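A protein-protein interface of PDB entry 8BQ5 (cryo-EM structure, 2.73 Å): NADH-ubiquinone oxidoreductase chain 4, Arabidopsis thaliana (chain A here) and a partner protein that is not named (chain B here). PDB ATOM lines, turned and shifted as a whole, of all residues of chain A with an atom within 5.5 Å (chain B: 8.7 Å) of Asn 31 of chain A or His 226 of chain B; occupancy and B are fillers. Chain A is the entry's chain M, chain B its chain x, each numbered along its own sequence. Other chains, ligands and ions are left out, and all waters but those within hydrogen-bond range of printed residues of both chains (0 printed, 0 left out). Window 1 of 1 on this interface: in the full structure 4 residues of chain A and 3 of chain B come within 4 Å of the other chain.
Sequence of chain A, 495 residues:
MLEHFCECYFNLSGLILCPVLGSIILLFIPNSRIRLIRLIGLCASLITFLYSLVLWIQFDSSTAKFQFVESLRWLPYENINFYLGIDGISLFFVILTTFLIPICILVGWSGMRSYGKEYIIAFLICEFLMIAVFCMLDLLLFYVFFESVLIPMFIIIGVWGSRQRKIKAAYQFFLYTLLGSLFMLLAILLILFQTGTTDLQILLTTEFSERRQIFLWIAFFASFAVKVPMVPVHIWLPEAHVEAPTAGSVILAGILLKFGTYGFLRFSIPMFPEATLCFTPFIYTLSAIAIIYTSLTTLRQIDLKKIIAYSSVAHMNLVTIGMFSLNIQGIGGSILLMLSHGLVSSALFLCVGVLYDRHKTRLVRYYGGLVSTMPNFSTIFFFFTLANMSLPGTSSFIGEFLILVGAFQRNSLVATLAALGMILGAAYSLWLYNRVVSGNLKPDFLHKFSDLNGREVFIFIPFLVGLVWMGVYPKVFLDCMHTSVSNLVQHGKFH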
ATOM      1  N   ILE A  29      18.497 -28.110  -5.155  1.00  0.00           N
ATOM      2  CA  ILE A  29      18.697 -26.924  -4.262  1.00  0.00           C
ATOM      3  C   ILE A  29      20.180 -26.837  -3.866  1.00  0.00           C
ATOM      4  O   ILE A  29      20.708 -27.831  -3.334  1.00  0.00           O
ATOM      5  CB  ILE A  29      17.729 -26.951  -3.055  1.00  0.00           C
ATOM      6  CG1 ILE A  29      16.402 -26.252  -3.365  1.00  0.00           C
ATOM      7  CG2 ILE A  29      18.370 -26.328  -1.830  1.00  0.00           C
ATOM      8  CD1 ILE A  29      15.653 -26.796  -4.554  1.00  0.00           C
ATOM      9  N   PRO A  30      20.879 -25.704  -4.127  1.00  0.00           N
ATOM     10  CA  PRO A  30      22.277 -25.549  -3.725  1.00  0.00           C
ATOM     11  C   PRO A  30      22.575 -25.967  -2.275  1.00  0.00           C
ATOM     12  O   PRO A  30      21.820 -25.608  -1.391  1.00  0.00           O
ATOM     13  CB  PRO A  30      22.552 -24.044  -3.910  1.00  0.00           C
ATOM     14  CG  PRO A  30      21.229 -23.418  -4.290  1.00  0.00           C
ATOM     15  CD  PRO A  30      20.386 -24.539  -4.851  1.00  0.00           C
ATOM     16  N   ASN A  31      23.670 -26.703  -2.062  1.00  0.00           N
ATOM     17  CA  ASN A  31      24.084 -27.107  -0.690  1.00  0.00           C
ATOM     18  C   ASN A  31      24.356 -25.864   0.162  1.00  0.00           C
ATOM     19  O   ASN A  31      24.332 -25.992   1.399  1.00  0.00           O
ATOM     20  CB  ASN A  31      25.289 -28.051  -0.717  1.00  0.00           C
ATOM     21  CG  ASN A  31      24.913 -29.516  -0.672  1.00  0.00           C
ATOM     22  OD1 ASN A  31      24.110 -29.936   0.161  1.00  0.00           O
ATOM     23  ND2 ASN A  31      25.513 -30.309  -1.544  1.00  0.00           N
ATOM     24  N   SER A  32      24.616 -24.710  -0.463  1.00  0.00           N
ATOM     25  CA  SER A  32      24.774 -23.441   0.301  1.00  0.00           C
ATOM     26  C   SER A  32      23.488 -23.085   1.064  1.00  0.00           C
ATOM     27  O   SER A  32      23.595 -22.324   2.034  1.00  0.00           O
ATOM     28  CB  SER A  32      25.180 -22.319  -0.612  1.00  0.00           C
ATOM     29  OG  SER A  32      24.167 -22.044  -1.565  1.00  0.00           O
ATOM     30  N   ARG A  33      22.324 -23.574   0.631  1.00  0.00           N
ATOM     31  CA  ARG A  33      21.029 -23.197   1.276  1.00  0.00           C
ATOM     32  C   ARG A  33      20.645 -24.232   2.345  1.00  0.00           C
ATOM     33  O   ARG A  33      19.589 -24.868   2.194  1.00  0.00           O
ATOM     34  CB  ARG A  33      19.953 -22.995   0.205  1.00  0.00           C
ATOM     35  CG  ARG A  33      20.403 -22.186  -1.003  1.00  0.00           C
ATOM     36  CD  ARG A  33      20.483 -20.690  -0.775  1.00  0.00           C
ATOM     37  NE  ARG A  33      21.800 -20.286  -0.301  1.00  0.00           N
ATOM     38  CZ  ARG A  33      22.486 -19.233  -0.732  1.00  0.00           C
ATOM     39  NH1 ARG A  33      21.989 -18.445  -1.669  1.00  0.00           N
ATOM     40  NH2 ARG A  33      23.674 -18.974  -0.217  1.00  0.00           N
ATOM     41  N   ILE A  34      21.457 -24.364   3.394  1.00  0.00           N
ATOM     42  CA  ILE A  34      21.218 -25.356   4.489  1.00  0.00           C
ATOM     43  C   ILE A  34      19.837 -25.160   5.131  1.00  0.00           C
ATOM     44  O   ILE A  34      19.129 -26.171   5.270  1.00  0.00           O
ATOM     45  CB  ILE A  34      22.352 -25.290   5.537  1.00  0.00           C
ATOM     46  CG1 ILE A  34      23.697 -25.742   4.960  1.00  0.00           C
ATOM     47  CG2 ILE A  34      21.985 -26.090   6.777  1.00  0.00           C
ATOM     48  CD1 ILE A  34      24.878 -25.451   5.853  1.00  0.00           C
ATOM     49  N   ILE A  37      17.019 -26.543   2.832  1.00  0.00           N
ATOM     50  CA  ILE A  37      17.118 -28.026   2.691  1.00  0.00           C
ATOM     51  C   ILE A  37      16.540 -28.696   3.938  1.00  0.00           C
ATOM     52  O   ILE A  37      15.706 -29.600   3.784  1.00  0.00           O
ATOM     53  CB  ILE A  37      18.595 -28.423   2.465  1.00  0.00           C
ATOM     54  CG1 ILE A  37      19.132 -27.894   1.135  1.00  0.00           C
ATOM     55  CG2 ILE A  37      18.786 -29.928   2.575  1.00  0.00           C
ATOM     56  CD1 ILE A  37      20.612 -28.117   0.937  1.00  0.00           C
ATOM     57  N   ARG A 113      24.890 -29.133   8.520  1.00  0.00           N
ATOM     58  CA  ARG A 113      25.801 -28.271   7.721  1.00  0.00           C
ATOM     59  C   ARG A 113      26.813 -29.179   7.016  1.00  0.00           C
ATOM     60  O   ARG A 113      27.054 -28.965   5.811  1.00  0.00           O
ATOM     61  CB  ARG A 113      26.497 -27.242   8.616  1.00  0.00           C
ATOM     62  CG  ARG A 113      27.357 -26.243   7.854  1.00  0.00           C
ATOM     63  CD  ARG A 113      28.074 -25.263   8.764  1.00  0.00           C
ATOM     64  NE  ARG A 113      27.146 -24.396   9.476  1.00  0.00           N
ATOM     65  CZ  ARG A 113      26.619 -23.276   8.988  1.00  0.00           C
ATOM     66  NH1 ARG A 113      26.927 -22.868   7.768  1.00  0.00           N
ATOM     67  NH2 ARG A 113      25.784 -22.567   9.724  1.00  0.00           N
ATOM     68  N   GLY A 116      24.332 -32.432   4.680  1.00  0.00           N
ATOM     69  CA  GLY A 116      23.927 -31.899   3.371  1.00  0.00           C
ATOM     70  C   GLY A 116      22.596 -32.450   2.916  1.00  0.00           C
ATOM     71  O   GLY A 116      21.899 -33.080   3.730  1.00  0.00           O
ATOM     72  N   LYS A 117      22.263 -32.230   1.644  1.00  0.00           N
ATOM     73  CA  LYS A 117      21.010 -32.781   1.086  1.00  0.00           C
ATOM     74  C   LYS A 117      21.160 -34.300   0.963  1.00  0.00           C
ATOM     75  O   LYS A 117      20.135 -34.975   1.075  1.00  0.00           O
ATOM     76  CB  LYS A 117      20.670 -32.076  -0.233  1.00  0.00           C
ATOM     77  CG  LYS A 117      21.776 -32.032  -1.276  1.00  0.00           C
ATOM     78  CD  LYS A 117      21.432 -31.123  -2.432  1.00  0.00           C
ATOM     79  CE  LYS A 117      22.475 -31.126  -3.527  1.00  0.00           C
ATOM     80  NZ  LYS A 117      22.151 -30.141  -4.584  1.00  0.00           N
ATOM     81  N   GLU A 118      22.387 -34.807   0.810  1.00  0.00           N
ATOM     82  CA  GLU A 118      22.614 -36.261   0.597  1.00  0.00           C
ATOM     83  C   GLU A 118      22.055 -37.044   1.787  1.00  0.00           C
ATOM     84  O   GLU A 118      21.492 -38.123   1.555  1.00  0.00           O
ATOM     85  CB  GLU A 118      24.107 -36.527   0.390  1.00  0.00           C
ATOM     86  CG  GLU A 118      24.727 -35.662  -0.693  1.00  0.00           C
ATOM     87  CD  GLU A 118      26.243 -35.544  -0.657  1.00  0.00           C
ATOM     88  OE1 GLU A 118      26.851 -35.980   0.343  1.00  0.00           O
ATOM     89  OE2 GLU A 118      26.813 -35.015  -1.632  1.00  0.00           O
ATOM     90  N   GLY B  93      36.366 -25.770  -6.576  1.00  0.00           N
ATOM     91  CA  GLY B  93      35.810 -25.302  -5.327  1.00  0.00           C
ATOM     92  C   GLY B  93      36.651 -24.285  -4.594  1.00  0.00           C
ATOM     93  O   GLY B  93      36.281 -23.885  -3.484  1.00  0.00           O
ATOM     94  N   SER B  95      38.617 -20.499  -4.103  1.00  0.00           N
ATOM     95  CA  SER B  95      38.263 -19.108  -4.350  1.00  0.00           C
ATOM     96  C   SER B  95      39.459 -18.210  -4.071  1.00  0.00           C
ATOM     97  O   SER B  95      40.212 -18.441  -3.123  1.00  0.00           O
ATOM     98  CB  SER B  95      37.064 -18.677  -3.498  1.00  0.00           C
ATOM     99  OG  SER B  95      37.231 -19.054  -2.145  1.00  0.00           O
ATOM    100  N   TRP B  97      40.195 -14.021  -3.781  1.00  0.00           N
ATOM    101  CA  TRP B  97      39.378 -12.839  -3.551  1.00  0.00           C
ATOM    102  C   TRP B  97      40.111 -11.559  -3.947  1.00  0.00           C
ATOM    103  O   TRP B  97      41.275 -11.575  -4.350  1.00  0.00           O
ATOM    104  CB  TRP B  97      38.931 -12.803  -2.088  1.00  0.00           C
ATOM    105  CG  TRP B  97      38.079 -13.989  -1.751  1.00  0.00           C
ATOM    106  CD1 TRP B  97      38.505 -15.261  -1.500  1.00  0.00           C
ATOM    107  CD2 TRP B  97      36.653 -14.019  -1.659  1.00  0.00           C
ATOM    108  NE1 TRP B  97      37.432 -16.078  -1.246  1.00  0.00           N
ATOM    109  CE2 TRP B  97      36.283 -15.340  -1.337  1.00  0.00           C
ATOM    110  CE3 TRP B  97      35.651 -13.056  -1.810  1.00  0.00           C
ATOM    111  CZ2 TRP B  97      34.955 -15.720  -1.165  1.00  0.00           C
ATOM    112  CZ3 TRP B  97      34.336 -13.436  -1.638  1.00  0.00           C
ATOM    113  CH2 TRP B  97      33.999 -14.755  -1.320  1.00  0.00           C
ATOM    114  N   CYS B 114      38.807 -26.799  -2.644  1.00  0.00           N
ATOM    115  CA  CYS B 114      37.994 -26.103  -1.644  1.00  0.00           C
ATOM    116  C   CYS B 114      38.828 -25.205  -0.729  1.00  0.00           C
ATOM    117  O   CYS B 114      38.414 -24.888   0.387  1.00  0.00           O
ATOM    118  CB  CYS B 114      37.177 -27.098  -0.813  1.00  0.00           C
ATOM    119  SG  CYS B 114      36.072 -26.343   0.396  1.00  0.00           S
ATOM    120  N   ASN B 116      40.825 -21.470  -0.002  1.00  0.00           N
ATOM    121  CA  ASN B 116      40.548 -20.078  -0.326  1.00  0.00           C
ATOM    122  C   ASN B 116      41.748 -19.200  -0.013  1.00  0.00           C
ATOM    123  O   ASN B 116      42.392 -19.352   1.029  1.00  0.00           O
ATOM    124  CB  ASN B 116      39.308 -19.558   0.419  1.00  0.00           C
ATOM    125  CG  ASN B 116      39.421 -19.702   1.919  1.00  0.00           C
ATOM    126  OD1 ASN B 116      39.926 -18.812   2.600  1.00  0.00           O
ATOM    127  ND2 ASN B 116      38.938 -20.819   2.447  1.00  0.00           N
ATOM    128  N   PRO B 218      37.768 -27.803   8.153  1.00  0.00           N
ATOM    129  CA  PRO B 218      37.147 -28.016   6.836  1.00  0.00           C
ATOM    130  C   PRO B 218      35.755 -27.424   6.745  1.00  0.00           C
ATOM    131  O   PRO B 218      35.312 -27.059   5.650  1.00  0.00           O
ATOM    132  CB  PRO B 218      37.134 -29.545   6.691  1.00  0.00           C
ATOM    133  CG  PRO B 218      37.301 -30.071   8.065  1.00  0.00           C
ATOM    134  CD  PRO B 218      38.148 -29.081   8.781  1.00  0.00           C
ATOM    135  N   LYS B 219      35.059 -27.298   7.876  1.00  0.00           N
ATOM    136  CA  LYS B 219      33.762 -26.630   7.881  1.00  0.00           C
ATOM    137  C   LYS B 219      33.903 -25.160   7.502  1.00  0.00           C
ATOM    138  O   LYS B 219      33.077 -24.621   6.756  1.00  0.00           O
ATOM    139  CB  LYS B 219      33.115 -26.777   9.255  1.00  0.00           C
ATOM    140  CG  LYS B 219      32.628 -28.182   9.546  1.00  0.00           C
ATOM    141  CD  LYS B 219      31.624 -28.193  10.680  1.00  0.00           C
ATOM    142  CE  LYS B 219      32.163 -28.965  11.869  1.00  0.00           C
ATOM    143  NZ  LYS B 219      31.496 -30.283  12.038  1.00  0.00           N
ATOM    144  N   LEU B 220      34.944 -24.495   8.008  1.00  0.00           N
ATOM    145  CA  LEU B 220      35.198 -23.112   7.617  1.00  0.00           C
ATOM    146  C   LEU B 220      35.511 -23.007   6.132  1.00  0.00           C
ATOM    147  O   LEU B 220      35.024 -22.095   5.448  1.00  0.00           O
ATOM    148  CB  LEU B 220      36.342 -22.531   8.445  1.00  0.00           C
ATOM    149  CG  LEU B 220      36.702 -21.080   8.125  1.00  0.00           C
ATOM    150  CD1 LEU B 220      35.478 -20.185   8.226  1.00  0.00           C
ATOM    151  CD2 LEU B 220      37.796 -20.592   9.048  1.00  0.00           C
ATOM    152  N   ALA B 221      36.331 -23.928   5.614  1.00  0.00           N
ATOM    153  CA  ALA B 221      36.619 -23.894   4.181  1.00  0.00           C
ATOM    154  C   ALA B 221      35.346 -24.074   3.356  1.00  0.00           C
ATOM    155  O   ALA B 221      35.134 -23.374   2.357  1.00  0.00           O
ATOM    156  CB  ALA B 221      37.652 -24.961   3.822  1.00  0.00           C
ATOM    157  N   VAL B 222      34.479 -25.000   3.773  1.00  0.00           N
ATOM    158  CA  VAL B 222      33.233 -25.244   3.050  1.00  0.00           C
ATOM    159  C   VAL B 222      32.332 -24.014   3.100  1.00  0.00           C
ATOM    160  O   VAL B 222      31.698 -23.651   2.103  1.00  0.00           O
ATOM    161  CB  VAL B 222      32.526 -26.491   3.616  1.00  0.00           C
ATOM    162  CG1 VAL B 222      31.061 -26.512   3.212  1.00  0.00           C
ATOM    163  CG2 VAL B 222      33.230 -27.754   3.149  1.00  0.00           C
ATOM    164  N   ALA B 223      32.258 -23.355   4.259  1.00  0.00           N
ATOM    165  CA  ALA B 223      31.425 -22.162   4.378  1.00  0.00           C
ATOM    166  C   ALA B 223      31.932 -21.038   3.482  1.00  0.00           C
ATOM    167  O   ALA B 223      31.139 -20.321   2.857  1.00  0.00           O
ATOM    168  CB  ALA B 223      31.370 -21.701   5.835  1.00  0.00           C
ATOM    169  N   ILE B 224      33.252 -20.863   3.409  1.00  0.00           N
ATOM    170  CA  ILE B 224      33.802 -19.818   2.550  1.00  0.00           C
ATOM    171  C   ILE B 224      33.548 -20.143   1.081  1.00  0.00           C
ATOM    172  O   ILE B 224      33.275 -19.247   0.271  1.00  0.00           O
ATOM    173  CB  ILE B 224      35.296 -19.609   2.854  1.00  0.00           C
ATOM    174  CG1 ILE B 224      35.457 -18.951   4.226  1.00  0.00           C
ATOM    175  CG2 ILE B 224      35.951 -18.744   1.790  1.00  0.00           C
ATOM    176  CD1 ILE B 224      36.878 -18.924   4.733  1.00  0.00           C
ATOM    177  N   ASN B 225      33.617 -21.425   0.712  1.00  0.00           N
ATOM    178  CA  ASN B 225      33.263 -21.812  -0.653  1.00  0.00           C
ATOM    179  C   ASN B 225      31.792 -21.514  -0.946  1.00  0.00           C
ATOM    180  O   ASN B 225      31.444 -21.039  -2.038  1.00  0.00           O
ATOM    181  CB  ASN B 225      33.580 -23.293  -0.870  1.00  0.00           C
ATOM    182  CG  ASN B 225      32.753 -23.917  -1.973  1.00  0.00           C
ATOM    183  OD1 ASN B 225      33.121 -23.868  -3.146  1.00  0.00           O
ATOM    184  ND2 ASN B 225      31.635 -24.525  -1.600  1.00  0.00           N
ATOM    185  N   HIS B 226      30.917 -21.781   0.027  1.00  0.00           N
ATOM    186  CA  HIS B 226      29.502 -21.469  -0.145  1.00  0.00           C
ATOM    187  C   HIS B 226      29.294 -19.978  -0.361  1.00  0.00           C
ATOM    188  O   HIS B 226      28.477 -19.572  -1.194  1.00  0.00           O
ATOM    189  CB  HIS B 226      28.704 -21.949   1.065  1.00  0.00           C
ATOM    190  CG  HIS B 226      28.482 -23.428   1.093  1.00  0.00           C
ATOM    191  ND1 HIS B 226      28.072 -24.097   2.225  1.00  0.00           N
ATOM    192  CD2 HIS B 226      28.624 -24.368   0.130  1.00  0.00           C
ATOM    193  CE1 HIS B 226      27.966 -25.386   1.957  1.00  0.00           C
ATOM    194  NE2 HIS B 226      28.296 -25.577   0.693  1.00  0.00           N
ATOM    195  N   LEU B 227      30.015 -19.146   0.391  1.00  0.00           N
ATOM    196  CA  LEU B 227      29.918 -17.705   0.171  1.00  0.00           C
ATOM    197  C   LEU B 227      30.423 -17.320  -1.216  1.00  0.00           C
ATOM    198  O   LEU B 227      29.815 -16.487  -1.896  1.00  0.00           O
ATOM    199  CB  LEU B 227      30.688 -16.943   1.246  1.00  0.00           C
ATOM    200  CG  LEU B 227      30.567 -15.421   1.135  1.00  0.00           C
ATOM    201  CD1 LEU B 227      29.111 -14.996   0.977  1.00  0.00           C
ATOM    202  CD2 LEU B 227      31.197 -14.741   2.329  1.00  0.00           C
ATOM    203  N   SER B 228      31.537 -17.914  -1.649  1.00  0.00           N
ATOM    204  CA  SER B 228      32.091 -17.581  -2.959  1.00  0.00           C
ATOM    205  C   SER B 228      31.144 -17.964  -4.089  1.00  0.00           C
ATOM    206  O   SER B 228      31.205 -17.375  -5.174  1.00  0.00           O
ATOM    207  CB  SER B 228      33.444 -18.266  -3.148  1.00  0.00           C
ATOM    208  OG  SER B 228      33.279 -19.611  -3.556  1.00  0.00           O
ATOM    209  N   GLY B 229      30.285 -18.961  -3.865  1.00  0.00           N
ATOM    210  CA  GLY B 229      29.302 -19.313  -4.883  1.00  0.00           C
ATOM    211  C   GLY B 229      28.350 -18.173  -5.208  1.00  0.00           C
ATOM    212  O   GLY B 229      27.943 -17.994  -6.362  1.00  0.00           O
ATOM    213  N   ASP B 230      27.987 -17.386  -4.194  1.00  0.00           N
ATOM    214  CA  ASP B 230      27.106 -16.210  -4.400  1.00  0.00           C
ATOM    215  C   ASP B 230      27.787 -15.197  -5.324  1.00  0.00           C
ATOM    216  O   ASP B 230      27.078 -14.585  -6.134  1.00  0.00           O
ATOM    217  CB  ASP B 230      26.744 -15.571  -3.062  1.00  0.00           C
ATOM    218  CG  ASP B 230      26.047 -16.527  -2.109  1.00  0.00           C
ATOM    219  OD1 ASP B 230      25.225 -17.340  -2.583  1.00  0.00           O
ATOM    220  OD2 ASP B 230      26.328 -16.452  -0.899  1.00  0.00           O
ATOM    221  N   TYR B 231      29.102 -15.012  -5.188  1.00  0.00           N
ATOM    222  CA  TYR B 231      29.825 -14.121  -6.088  1.00  0.00           C
ATOM    223  C   TYR B 231      29.956 -14.726  -7.477  1.00  0.00           C
ATOM    224  O   TYR B 231      29.852 -14.015  -8.484  1.00  0.00           O
ATOM    225  CB  TYR B 231      31.202 -13.805  -5.517  1.00  0.00           C
ATOM    226  CG  TYR B 231      31.156 -12.839  -4.371  1.00  0.00           C
ATOM    227  CD1 TYR B 231      30.897 -13.280  -3.084  1.00  0.00           C
ATOM    228  CD2 TYR B 231      31.364 -11.484  -4.574  1.00  0.00           C
ATOM    229  CE1 TYR B 231      30.847 -12.404  -2.031  1.00  0.00           C
ATOM    230  CE2 TYR B 231      31.318 -10.599  -3.525  1.00  0.00           C
ATOM    231  CZ  TYR B 231      31.058 -11.065  -2.254  1.00  0.00           C
ATOM    232  OH  TYR B 231      31.007 -10.194  -1.193  1.00  0.00           O
ATOM    233  N   PHE B 232      30.196 -16.036  -7.547  1.00  0.00           N
ATOM    234  CA  PHE B 232      30.324 -16.707  -8.835  1.00  0.00           C
ATOM    235  C   PHE B 232      29.059 -16.545  -9.664  1.00  0.00           C
ATOM    236  O   PHE B 232      29.126 -16.321 -10.879  1.00  0.00           O
ATOM    237  CB  PHE B 232      30.633 -18.188  -8.621  1.00  0.00           C
ATOM    238  CG  PHE B 232      30.972 -18.930  -9.880  1.00  0.00           C
ATOM    239  CD1 PHE B 232      29.976 -19.481 -10.668  1.00  0.00           C
ATOM    240  CD2 PHE B 232      32.289 -19.094 -10.266  1.00  0.00           C
ATOM    241  CE1 PHE B 232      30.286 -20.166 -11.825  1.00  0.00           C
ATOM    242  CE2 PHE B 232      32.606 -19.781 -11.419  1.00  0.00           C
ATOM    243  CZ  PHE B 232      31.603 -20.317 -12.200  1.00  0.00           C
ATOM    244  N   SER B 233      27.892 -16.517  -9.033  1.00  0.00           N
ATOM    245  CA  SER B 233      26.626 -16.454  -9.812  1.00  0.00           C
ATOM    246  C   SER B 233      26.354 -15.041 -10.343  1.00  0.00           C
ATOM    247  O   SER B 233      25.440 -14.904 -11.160  1.00  0.00           O
ATOM    248  CB  SER B 233      25.475 -16.966  -9.001  1.00  0.00           C
ATOM    249  OG  SER B 233      25.710 -18.304  -8.592  1.00  0.00           O
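The guanidinium group of Arg 33 of chain A lies within salt-bridge range of the side-chain carboxylate of Asp 230 of chain B, at 3.3 Å.
OD1 of Asn 31 of chain A lies within hydrogen-bond range of N of Lys 117 of chain A, at 3.3 Å.
The side-chain hydroxyl (OG) of Ser 32 of chain A sits at hydrogen-bond distance from the guanidinium group (NE) of Arg 33 of chain A (3.2 Å).
Asn 31 of chain A touches His 226 of chain B.
CA of Ser 32 of chain A touches CG of His 226 of chain B, at 3.8 Å.
Asn 31 of chain A touches just one residue of chain B: His 226.
His 226 of chain B touches just these residues of chain A: Asn 31 and Ser 32.
Ser 32 of chain A touches just one residue of chain B: His 226.
Of the printed residues of chain B, Arg 33 of chain A touches Asp 230.
Of the printed residues of chain A, Asp 230 of chain B touches Arg 33.
Lys 219 of chain B touches none of the printed residues of chain A.
Pro 218 of chain B touches none of the printed residues of chain A.
The nearest residue of chain B that does not touch Asn 31 of chain A is Val 222 of chain B (7.0 Å).
The nearest residue of chain A that does not touch His 226 of chain B is Arg 33 of chain A (4.9 Å).
Hydrophobic or aromatic side chains of chain B that line the printed part of chain A: His 226.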
